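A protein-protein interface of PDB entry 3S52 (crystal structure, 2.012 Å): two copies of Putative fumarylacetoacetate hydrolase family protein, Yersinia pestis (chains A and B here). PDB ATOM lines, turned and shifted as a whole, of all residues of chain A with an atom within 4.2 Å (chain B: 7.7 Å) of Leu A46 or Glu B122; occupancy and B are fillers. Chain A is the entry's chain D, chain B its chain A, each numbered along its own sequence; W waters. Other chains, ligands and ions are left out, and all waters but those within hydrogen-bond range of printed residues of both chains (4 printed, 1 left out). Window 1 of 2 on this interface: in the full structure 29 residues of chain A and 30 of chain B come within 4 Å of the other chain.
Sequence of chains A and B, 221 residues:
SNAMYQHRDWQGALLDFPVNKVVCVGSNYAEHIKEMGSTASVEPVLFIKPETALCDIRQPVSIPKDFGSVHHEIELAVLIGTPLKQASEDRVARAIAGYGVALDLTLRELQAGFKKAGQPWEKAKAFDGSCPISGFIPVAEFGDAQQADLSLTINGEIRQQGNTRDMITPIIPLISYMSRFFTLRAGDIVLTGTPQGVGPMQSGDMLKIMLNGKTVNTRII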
ATOM      1  N   CYS A  24     -25.489  -2.352  -5.246  1.00  0.00           N
ATOM      2  CA  CYS A  24     -26.311  -3.098  -4.295  1.00  0.00           C
ATOM      3  C   CYS A  24     -27.178  -2.163  -3.478  1.00  0.00           C
ATOM      4  O   CYS A  24     -26.818  -1.010  -3.275  1.00  0.00           O
ATOM      5  CB  CYS A  24     -25.421  -3.871  -3.318  1.00  0.00           C
ATOM      6  SG  CYS A  24     -24.087  -4.839  -4.061  1.00  0.00           S
ATOM      7  N   PRO A  44     -33.362   4.749  -1.241  1.00  0.00           N
ATOM      8  CA  PRO A  44     -32.664   3.465  -1.137  1.00  0.00           C
ATOM      9  C   PRO A  44     -31.241   3.611  -0.593  1.00  0.00           C
ATOM     10  O   PRO A  44     -30.539   4.546  -0.968  1.00  0.00           O
ATOM     11  CB  PRO A  44     -32.629   2.989  -2.584  1.00  0.00           C
ATOM     12  CG  PRO A  44     -33.882   3.539  -3.161  1.00  0.00           C
ATOM     13  CD  PRO A  44     -34.047   4.898  -2.533  1.00  0.00           C
ATOM     14  N   VAL A  45     -30.843   2.713   0.305  1.00  0.00           N
ATOM     15  CA  VAL A  45     -29.464   2.645   0.774  1.00  0.00           C
ATOM     16  C   VAL A  45     -28.639   1.906  -0.282  1.00  0.00           C
ATOM     17  O   VAL A  45     -28.955   0.773  -0.627  1.00  0.00           O
ATOM     18  CB  VAL A  45     -29.377   1.897   2.118  1.00  0.00           C
ATOM     19  CG1 VAL A  45     -27.936   1.723   2.550  1.00  0.00           C
ATOM     20  CG2 VAL A  45     -30.184   2.634   3.201  1.00  0.00           C
ATOM     21  N   LEU A  46     -27.599   2.554  -0.801  1.00  0.00           N
ATOM     22  CA  LEU A  46     -26.809   1.991  -1.881  1.00  0.00           C
ATOM     23  C   LEU A  46     -25.342   1.794  -1.507  1.00  0.00           C
ATOM     24  O   LEU A  46     -24.707   2.664  -0.898  1.00  0.00           O
ATOM     25  CB  LEU A  46     -26.878   2.877  -3.133  1.00  0.00           C
ATOM     26  CG  LEU A  46     -28.245   3.173  -3.772  1.00  0.00           C
ATOM     27  CD1 LEU A  46     -28.054   3.910  -5.077  1.00  0.00           C
ATOM     28  CD2 LEU A  46     -29.032   1.900  -4.011  1.00  0.00           C
ATOM     29  N   PHE A  47     -24.798   0.655  -1.895  1.00  0.00           N
ATOM     30  CA  PHE A  47     -23.367   0.440  -1.763  1.00  0.00           C
ATOM     31  C   PHE A  47     -22.919  -0.399  -2.937  1.00  0.00           C
ATOM     32  O   PHE A  47     -23.750  -0.851  -3.724  1.00  0.00           O
ATOM     33  CB  PHE A  47     -23.023  -0.225  -0.427  1.00  0.00           C
ATOM     34  CG  PHE A  47     -23.635  -1.597  -0.249  1.00  0.00           C
ATOM     35  CD1 PHE A  47     -24.899  -1.742   0.303  1.00  0.00           C
ATOM     36  CD2 PHE A  47     -22.938  -2.737  -0.628  1.00  0.00           C
ATOM     37  CE1 PHE A  47     -25.459  -2.992   0.458  1.00  0.00           C
ATOM     38  CE2 PHE A  47     -23.496  -3.996  -0.475  1.00  0.00           C
ATOM     39  CZ  PHE A  47     -24.752  -4.125   0.067  1.00  0.00           C
ATOM     40  N   ILE A  48     -21.616  -0.630  -3.036  1.00  0.00           N
ATOM     41  CA  ILE A  48     -21.029  -1.202  -4.233  1.00  0.00           C
ATOM     42  C   ILE A  48     -19.984  -2.228  -3.845  1.00  0.00           C
ATOM     43  O   ILE A  48     -19.297  -2.061  -2.840  1.00  0.00           O
ATOM     44  CB  ILE A  48     -20.351  -0.121  -5.088  1.00  0.00           C
ATOM     45  CG1 ILE A  48     -21.384   0.860  -5.638  1.00  0.00           C
ATOM     46  CG2 ILE A  48     -19.604  -0.737  -6.256  1.00  0.00           C
ATOM     47  CD1 ILE A  48     -20.771   1.965  -6.472  1.00  0.00           C
ATOM     48  N   GLU A 122     -17.299  -0.592   3.192  1.00  0.00           N
ATOM     49  CA  GLU A 122     -16.522  -1.380   2.244  1.00  0.00           C
ATOM     50  C   GLU A 122     -15.833  -2.592   2.847  1.00  0.00           C
ATOM     51  O   GLU A 122     -15.885  -3.690   2.270  1.00  0.00           O
ATOM     52  CB  GLU A 122     -15.489  -0.513   1.534  1.00  0.00           C
ATOM     53  CG  GLU A 122     -16.028   0.155   0.294  1.00  0.00           C
ATOM     54  CD  GLU A 122     -16.705   1.462   0.596  1.00  0.00           C
ATOM     55  OE1 GLU A 122     -16.978   1.741   1.786  1.00  0.00           O
ATOM     56  OE2 GLU A 122     -16.943   2.226  -0.360  1.00  0.00           O
ATOM     57  N   TYR A 177     -33.042   4.658 -10.076  1.00  0.00           N
ATOM     58  CA  TYR A 177     -32.461   5.467  -9.000  1.00  0.00           C
ATOM     59  C   TYR A 177     -30.930   5.349  -8.932  1.00  0.00           C
ATOM     60  O   TYR A 177     -30.205   6.352  -8.905  1.00  0.00           O
ATOM     61  CB  TYR A 177     -33.081   5.059  -7.666  1.00  0.00           C
ATOM     62  CG  TYR A 177     -32.554   5.814  -6.465  1.00  0.00           C
ATOM     63  CD1 TYR A 177     -33.003   7.103  -6.166  1.00  0.00           C
ATOM     64  CD2 TYR A 177     -31.633   5.229  -5.615  1.00  0.00           C
ATOM     65  CE1 TYR A 177     -32.533   7.783  -5.067  1.00  0.00           C
ATOM     66  CE2 TYR A 177     -31.157   5.899  -4.520  1.00  0.00           C
ATOM     67  CZ  TYR A 177     -31.608   7.171  -4.245  1.00  0.00           C
ATOM     68  OH  TYR A 177     -31.117   7.817  -3.139  1.00  0.00           O
ATOM     69  N   MET A 178     -30.435   4.118  -8.916  1.00  0.00           N
ATOM     70  CA  MET A 178     -28.987   3.884  -8.894  1.00  0.00           C
ATOM     71  C   MET A 178     -28.233   4.654  -9.974  1.00  0.00           C
ATOM     72  O   MET A 178     -27.150   5.184  -9.722  1.00  0.00           O
ATOM     73  CB  MET A 178     -28.692   2.401  -9.070  1.00  0.00           C
ATOM     74  CG  MET A 178     -29.026   1.562  -7.867  1.00  0.00           C
ATOM     75  SD  MET A 178     -28.972  -0.352  -8.311  1.00  0.00           S
ATOM     76  CE  MET A 178     -29.023  -1.064  -6.497  1.00  0.00           C
ATOM     77  N   PHE A 182     -24.501   6.364 -10.093  1.00  0.00           N
ATOM     78  CA  PHE A 182     -23.424   5.640 -10.752  1.00  0.00           C
ATOM     79  C   PHE A 182     -23.825   5.167 -12.143  1.00  0.00           C
ATOM     80  O   PHE A 182     -24.855   4.526 -12.301  1.00  0.00           O
ATOM     81  CB  PHE A 182     -23.041   4.437  -9.898  1.00  0.00           C
ATOM     82  CG  PHE A 182     -23.223   4.659  -8.420  1.00  0.00           C
ATOM     83  CD1 PHE A 182     -22.299   5.392  -7.696  1.00  0.00           C
ATOM     84  CD2 PHE A 182     -24.302   4.113  -7.755  1.00  0.00           C
ATOM     85  CE1 PHE A 182     -22.468   5.594  -6.325  1.00  0.00           C
ATOM     86  CE2 PHE A 182     -24.471   4.308  -6.384  1.00  0.00           C
ATOM     87  CZ  PHE A 182     -23.554   5.054  -5.674  1.00  0.00           C
ATOM     88  N   PHE B  47     -12.589   3.079   2.048  1.00  0.00           N
ATOM     89  CA  PHE B  47     -13.731   3.012   1.146  1.00  0.00           C
ATOM     90  C   PHE B  47     -13.184   2.924  -0.261  1.00  0.00           C
ATOM     91  O   PHE B  47     -11.969   3.017  -0.456  1.00  0.00           O
ATOM     92  CB  PHE B  47     -14.656   4.219   1.325  1.00  0.00           C
ATOM     93  CG  PHE B  47     -13.989   5.547   1.049  1.00  0.00           C
ATOM     94  CD1 PHE B  47     -13.285   6.208   2.043  1.00  0.00           C
ATOM     95  CD2 PHE B  47     -14.090   6.140  -0.201  1.00  0.00           C
ATOM     96  CE1 PHE B  47     -12.674   7.429   1.790  1.00  0.00           C
ATOM     97  CE2 PHE B  47     -13.478   7.364  -0.472  1.00  0.00           C
ATOM     98  CZ  PHE B  47     -12.768   8.006   0.518  1.00  0.00           C
ATOM     99  N   ILE B  48     -14.062   2.761  -1.244  1.00  0.00           N
ATOM    100  CA  ILE B  48     -13.605   2.452  -2.601  1.00  0.00           C
ATOM    101  C   ILE B  48     -14.398   3.270  -3.611  1.00  0.00           C
ATOM    102  O   ILE B  48     -15.576   3.524  -3.389  1.00  0.00           O
ATOM    103  CB  ILE B  48     -13.792   0.944  -2.917  1.00  0.00           C
ATOM    104  CG1 ILE B  48     -12.951   0.086  -1.966  1.00  0.00           C
ATOM    105  CG2 ILE B  48     -13.438   0.628  -4.399  1.00  0.00           C
ATOM    106  CD1 ILE B  48     -13.083  -1.433  -2.189  1.00  0.00           C
ATOM    107  N   LYS B  49     -13.750   3.682  -4.703  1.00  0.00           N
ATOM    108  CA  LYS B  49     -14.438   4.307  -5.820  1.00  0.00           C
ATOM    109  C   LYS B  49     -14.325   3.380  -7.030  1.00  0.00           C
ATOM    110  O   LYS B  49     -13.304   2.707  -7.212  1.00  0.00           O
ATOM    111  CB  LYS B  49     -13.809   5.649  -6.184  1.00  0.00           C
ATOM    112  CG  LYS B  49     -13.699   6.685  -5.062  1.00  0.00           C
ATOM    113  CD  LYS B  49     -13.145   8.000  -5.648  1.00  0.00           C
ATOM    114  CE  LYS B  49     -12.916   9.080  -4.605  1.00  0.00           C
ATOM    115  NZ  LYS B  49     -14.117   9.953  -4.379  1.00  0.00           N
ATOM    116  N   PRO B  50     -15.368   3.340  -7.871  1.00  0.00           N
ATOM    117  CA  PRO B  50     -15.318   2.410  -9.005  1.00  0.00           C
ATOM    118  C   PRO B  50     -14.709   3.071 -10.230  1.00  0.00           C
ATOM    119  O   PRO B  50     -14.443   4.268 -10.204  1.00  0.00           O
ATOM    120  CB  PRO B  50     -16.796   2.119  -9.256  1.00  0.00           C
ATOM    121  CG  PRO B  50     -17.471   3.433  -8.903  1.00  0.00           C
ATOM    122  CD  PRO B  50     -16.689   3.991  -7.736  1.00  0.00           C
ATOM    123  N   LEU B 107     -19.608  14.569  -1.797  1.00  0.00           N
ATOM    124  CA  LEU B 107     -20.803  15.366  -1.587  1.00  0.00           C
ATOM    125  C   LEU B 107     -20.894  15.441  -0.084  1.00  0.00           C
ATOM    126  O   LEU B 107     -21.414  14.547   0.579  1.00  0.00           O
ATOM    127  CB  LEU B 107     -22.018  14.655  -2.188  1.00  0.00           C
ATOM    128  CG  LEU B 107     -21.926  14.524  -3.719  1.00  0.00           C
ATOM    129  CD1 LEU B 107     -23.022  13.622  -4.310  1.00  0.00           C
ATOM    130  CD2 LEU B 107     -21.956  15.897  -4.360  1.00  0.00           C
ATOM    131  N   LEU B 110     -24.284  15.129   1.939  1.00  0.00           N
ATOM    132  CA  LEU B 110     -24.754  13.738   1.952  1.00  0.00           C
ATOM    133  C   LEU B 110     -23.889  12.892   2.875  1.00  0.00           C
ATOM    134  O   LEU B 110     -24.407  12.160   3.723  1.00  0.00           O
ATOM    135  CB  LEU B 110     -24.749  13.122   0.550  1.00  0.00           C
ATOM    136  CG  LEU B 110     -25.895  13.383  -0.421  1.00  0.00           C
ATOM    137  CD1 LEU B 110     -25.739  12.495  -1.652  1.00  0.00           C
ATOM    138  CD2 LEU B 110     -27.232  13.132   0.241  1.00  0.00           C
ATOM    139  N   PHE B 114     -24.973  10.410   5.900  1.00  0.00           N
ATOM    140  CA  PHE B 114     -24.620   8.989   5.938  1.00  0.00           C
ATOM    141  C   PHE B 114     -23.935   8.618   7.258  1.00  0.00           C
ATOM    142  O   PHE B 114     -24.271   7.601   7.867  1.00  0.00           O
ATOM    143  CB  PHE B 114     -23.759   8.583   4.708  1.00  0.00           C
ATOM    144  CG  PHE B 114     -24.471   8.769   3.402  1.00  0.00           C
ATOM    145  CD1 PHE B 114     -25.855   8.704   3.354  1.00  0.00           C
ATOM    146  CD2 PHE B 114     -23.778   9.066   2.239  1.00  0.00           C
ATOM    147  CE1 PHE B 114     -26.534   8.894   2.168  1.00  0.00           C
ATOM    148  CE2 PHE B 114     -24.453   9.263   1.045  1.00  0.00           C
ATOM    149  CZ  PHE B 114     -25.836   9.179   1.013  1.00  0.00           C
ATOM    150  N   GLN B 119     -24.820   4.874   7.475  1.00  0.00           N
ATOM    151  CA  GLN B 119     -25.140   4.365   6.135  1.00  0.00           C
ATOM    152  C   GLN B 119     -23.877   4.352   5.268  1.00  0.00           C
ATOM    153  O   GLN B 119     -22.905   5.011   5.602  1.00  0.00           O
ATOM    154  CB  GLN B 119     -26.207   5.235   5.479  1.00  0.00           C
ATOM    155  CG  GLN B 119     -27.630   5.013   6.017  1.00  0.00           C
ATOM    156  CD  GLN B 119     -28.686   5.773   5.218  1.00  0.00           C
ATOM    157  OE1 GLN B 119     -28.387   6.378   4.190  1.00  0.00           O
ATOM    158  NE2 GLN B 119     -29.927   5.735   5.687  1.00  0.00           N
ATOM    159  N   PRO B 120     -23.864   3.548   4.197  1.00  0.00           N
ATOM    160  CA  PRO B 120     -22.670   3.464   3.348  1.00  0.00           C
ATOM    161  C   PRO B 120     -22.401   4.793   2.641  1.00  0.00           C
ATOM    162  O   PRO B 120     -23.311   5.603   2.466  1.00  0.00           O
ATOM    163  CB  PRO B 120     -23.025   2.363   2.343  1.00  0.00           C
ATOM    164  CG  PRO B 120     -24.504   2.291   2.364  1.00  0.00           C
ATOM    165  CD  PRO B 120     -24.912   2.610   3.761  1.00  0.00           C
ATOM    166  N   TRP B 121     -21.151   5.027   2.263  1.00  0.00           N
ATOM    167  CA  TRP B 121     -20.769   6.341   1.762  1.00  0.00           C
ATOM    168  C   TRP B 121     -20.822   6.476   0.241  1.00  0.00           C
ATOM    169  O   TRP B 121     -20.600   7.573  -0.281  1.00  0.00           O
ATOM    170  CB  TRP B 121     -19.355   6.682   2.223  1.00  0.00           C
ATOM    171  CG  TRP B 121     -19.170   6.957   3.679  1.00  0.00           C
ATOM    172  CD1 TRP B 121     -20.088   6.805   4.693  1.00  0.00           C
ATOM    173  CD2 TRP B 121     -17.969   7.441   4.289  1.00  0.00           C
ATOM    174  NE1 TRP B 121     -19.518   7.176   5.893  1.00  0.00           N
ATOM    175  CE2 TRP B 121     -18.220   7.562   5.671  1.00  0.00           C
ATOM    176  CE3 TRP B 121     -16.694   7.762   3.796  1.00  0.00           C
ATOM    177  CZ2 TRP B 121     -17.246   8.005   6.568  1.00  0.00           C
ATOM    178  CZ3 TRP B 121     -15.727   8.208   4.686  1.00  0.00           C
ATOM    179  CH2 TRP B 121     -16.005   8.315   6.058  1.00  0.00           C
ATOM    180  N   GLU B 122     -21.097   5.377  -0.465  1.00  0.00           N
ATOM    181  CA  GLU B 122     -20.945   5.337  -1.928  1.00  0.00           C
ATOM    182  C   GLU B 122     -21.614   6.485  -2.683  1.00  0.00           C
ATOM    183  O   GLU B 122     -21.053   7.021  -3.640  1.00  0.00           O
ATOM    184  CB  GLU B 122     -21.444   4.003  -2.506  1.00  0.00           C
ATOM    185  CG  GLU B 122     -20.402   2.878  -2.465  1.00  0.00           C
ATOM    186  CD  GLU B 122     -20.368   2.145  -1.129  1.00  0.00           C
ATOM    187  OE1 GLU B 122     -20.863   2.703  -0.115  1.00  0.00           O
ATOM    188  OE2 GLU B 122     -19.869   0.999  -1.109  1.00  0.00           O
ATOM    189  N   LYS B 123     -22.832   6.842  -2.292  1.00  0.00           N
ATOM    190  CA  LYS B 123     -23.504   7.916  -3.005  1.00  0.00           C
ATOM    191  C   LYS B 123     -22.734   9.225  -2.874  1.00  0.00           C
ATOM    192  O   LYS B 123     -22.770  10.058  -3.784  1.00  0.00           O
ATOM    193  CB  LYS B 123     -24.966   8.098  -2.545  1.00  0.00           C
ATOM    194  CG  LYS B 123     -25.909   6.973  -2.949  1.00  0.00           C
ATOM    195  CD  LYS B 123     -27.396   7.341  -2.696  1.00  0.00           C
ATOM    196  CE  LYS B 123     -27.880   6.883  -1.347  1.00  0.00           C
ATOM    197  NZ  LYS B 123     -29.358   7.090  -1.205  1.00  0.00           N
ATOM    198  N   ALA B 124     -22.093   9.436  -1.722  1.00  0.00           N
ATOM    199  CA  ALA B 124     -21.303  10.654  -1.497  1.00  0.00           C
ATOM    200  C   ALA B 124     -19.877  10.614  -2.050  1.00  0.00           C
ATOM    201  O   ALA B 124     -19.271  11.666  -2.303  1.00  0.00           O
ATOM    202  CB  ALA B 124     -21.268  11.010  -0.018  1.00  0.00           C
ATOM    203  N   LYS B 125     -19.291   9.427  -2.064  1.00  0.00           N
ATOM    204  CA  LYS B 125     -17.901   9.266  -2.508  1.00  0.00           C
ATOM    205  C   LYS B 125     -17.624   8.599  -3.857  1.00  0.00           C
ATOM    206  O   LYS B 125     -16.519   8.721  -4.408  1.00  0.00           O
ATOM    207  CB  LYS B 125     -17.156   8.484  -1.422  1.00  0.00           C
ATOM    208  CG  LYS B 125     -17.019   9.242  -0.118  1.00  0.00           C
ATOM    209  CD  LYS B 125     -15.807  10.148  -0.209  1.00  0.00           C
ATOM    210  CE  LYS B 125     -15.394  10.709   1.130  1.00  0.00           C
ATOM    211  NZ  LYS B 125     -14.200  11.599   0.919  1.00  0.00           N
ATOM    212  N   ALA B 126     -18.600   7.834  -4.339  1.00  0.00           N
ATOM    213  CA  ALA B 126     -18.411   6.965  -5.512  1.00  0.00           C
ATOM    214  C   ALA B 126     -19.083   7.427  -6.794  1.00  0.00           C
ATOM    215  O   ALA B 126     -19.031   6.722  -7.807  1.00  0.00           O
ATOM    216  CB  ALA B 126     -18.803   5.523  -5.193  1.00  0.00           C
ATOM    217  N   PHE B 127     -19.740   8.583  -6.749  1.00  0.00           N
ATOM    218  CA  PHE B 127     -20.568   9.033  -7.861  1.00  0.00           C
ATOM    219  C   PHE B 127     -19.711   9.275  -9.113  1.00  0.00           C
ATOM    220  O   PHE B 127     -18.484   9.412  -9.023  1.00  0.00           O
ATOM    221  CB  PHE B 127     -21.343  10.306  -7.479  1.00  0.00           C
ATOM    222  CG  PHE B 127     -20.456  11.460  -7.091  1.00  0.00           C
ATOM    223  CD1 PHE B 127     -20.015  12.368  -8.046  1.00  0.00           C
ATOM    224  CD2 PHE B 127     -20.055  11.626  -5.771  1.00  0.00           C
ATOM    225  CE1 PHE B 127     -19.177  13.430  -7.680  1.00  0.00           C
ATOM    226  CE2 PHE B 127     -19.216  12.671  -5.401  1.00  0.00           C
ATOM    227  CZ  PHE B 127     -18.778  13.576  -6.351  1.00  0.00           C
ATOM    228  N   ASP B 128     -20.351   9.305 -10.281  1.00  0.00           N
ATOM    229  CA  ASP B 128     -19.616   9.467 -11.536  1.00  0.00           C
ATOM    230  C   ASP B 128     -18.709  10.676 -11.480  1.00  0.00           C
ATOM    231  O   ASP B 128     -19.137  11.750 -11.065  1.00  0.00           O
ATOM    232  CB  ASP B 128     -20.571   9.660 -12.720  1.00  0.00           C
ATOM    233  CG  ASP B 128     -21.303   8.390 -13.098  1.00  0.00           C
ATOM    234  OD1 ASP B 128     -20.986   7.316 -12.526  1.00  0.00           O
ATOM    235  OD2 ASP B 128     -22.183   8.469 -13.988  1.00  0.00           O
ATOM    236  N   SER B 130     -16.176  11.301  -9.568  1.00  0.00           N
ATOM    237  CA  SER B 130     -15.768  11.787  -8.237  1.00  0.00           C
ATOM    238  C   SER B 130     -14.266  11.628  -7.973  1.00  0.00           C
ATOM    239  O   SER B 130     -13.796  11.843  -6.852  1.00  0.00           O
ATOM    240  CB  SER B 130     -16.522  11.065  -7.129  1.00  0.00           C
ATOM    241  OG  SER B 130     -16.152   9.706  -7.125  1.00  0.00           O
HETATM  242  O   HOH W   1     -19.188  -1.398   0.091  1.00  0.00           O
HETATM  243  O   HOH W   2     -24.379   5.473  -0.160  1.00  0.00           O
HETATM  244  O   HOH W   3     -17.439   4.835  -1.223  1.00  0.00           O
HETATM  245  O   HOH W   4     -19.565   2.715   2.343  1.00  0.00           O
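The backbone NH (N) of Ile B48 sits at hydrogen-bond distance from the side-chain carboxylate (OE2) of Glu A122 (3.1 Å). The backbone carbonyl oxygen (O) of Pro A44 lies within hydrogen-bond range of the side-chain amino group (NZ) of Lys B123 (2.8 Å). OE2 of Glu A122 sits close to OE2 of Glu B122 (3.3 Å). The backbone NH of Ile A48 is in hydrogen-bond range of the side-chain carboxylate of Glu B122 (3.1 Å). The side-chain hydroxyl (OH) of Tyr A177 sits at hydrogen-bond distance from the side-chain amino group (NZ) of Lys B123 (2.7 Å).
CG2 of Val A45 touches NE2 of Gln B119, at 3.98 Å. Leu A46 touches Pro B120 (O to CG, 3.3 Å). Leu A46 touches Glu B122. CB of Phe A47 touches CB of Pro B120 (3.8 Å). Glu B122 touches Phe A47 (OE2 to CB, 3.5 Å). Glu A122 touches Phe B47. O of Glu B122 touches CE1 of Phe A182 (3.4 Å). CZ of Phe A182 touches N of Lys B123, at 3.9 Å. CD1 of Phe A182 touches O of Ala B126, at 3.5 Å. Phe A182 touches Asp B128.
Printed residues of chain B within 4 Å of Pro A44: Lys B123. Of the printed residues of chain B, Leu A46 touches Pro B120 and Glu B122. Of the printed residues of chain A, Ile B48 touches Glu A122. Of the printed residues of chain A, Gln B119 touches Val A45. Glu B122 touches five residues of chain A. Lys B125 touches none of the printed residues of chain A. Printed residues of chain A within 4 Å of Asp B128: Phe A182. The nearest printed residue of chain A that does not touch Glu B122 is Cys A24 (7.4 Å). The nearest printed residue of chain A that does not touch Pro B120 is Glu A122 (6.1 Å).
Phe A47 touches Glu B122, and with the chains exchanged Glu A122 touches Phe B47. Ile A48 touches Glu B122, and with the chains exchanged Glu A122 touches Ile B48. Glu B122 touches its own counterpart, Glu A122. 3 positions are printed for both chains. Of the 16 pairs that touch across the chains among the printed residues, 5 have their exchanged pair printed and touching as well.
Water W1 lies within hydrogen-bond range of the side-chain carboxylate (OE2) of Glu B122 and the backbone carbonyl oxygen (O) of Ile A48. Water W4 lies within hydrogen-bond range of the side-chain carboxylate of Glu B122 (2.8 Å), the backbone NH of Trp B121 (2.8 Å) and the side-chain carboxylate of Glu A122 (2.8 Å). Water W3 lies within hydrogen-bond range of the side-chain carboxylate of Glu A122 (2.8 Å) and the backbone carbonyl oxygen of Ile B48 (3.1 Å). Water W2 lies within hydrogen-bond range of O of Pro B120 (2.8 Å), O of Leu A46 (2.9 Å), N of Lys B123 (3.0 Å) and N of Glu B122 (3.3 Å).
Hydrophobic or aromatic side chains of chain B within 4 Å of the printed part of chain A: Phe B47, Ile B48, Pro B120 and Ala B126. Hydrophobic or aromatic side chains of chain A within 4 Å of the printed part of chain B: Val A45, Phe A47, Ile A48, Tyr A177 and Phe A182. Among the printed residues, no Asp or Glu carboxylate lies within 4 Å of a Lys or Arg side-chain nitrogen of the other chain.
The backbone NH of Cys A24 lies within hydrogen-bond range of the backbone carbonyl oxygen of Phe A47 (2.8 Å). The backbone carbonyl oxygen (O) of Phe B114 lies within hydrogen-bond range of the backbone NH (N) of Gln B119.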
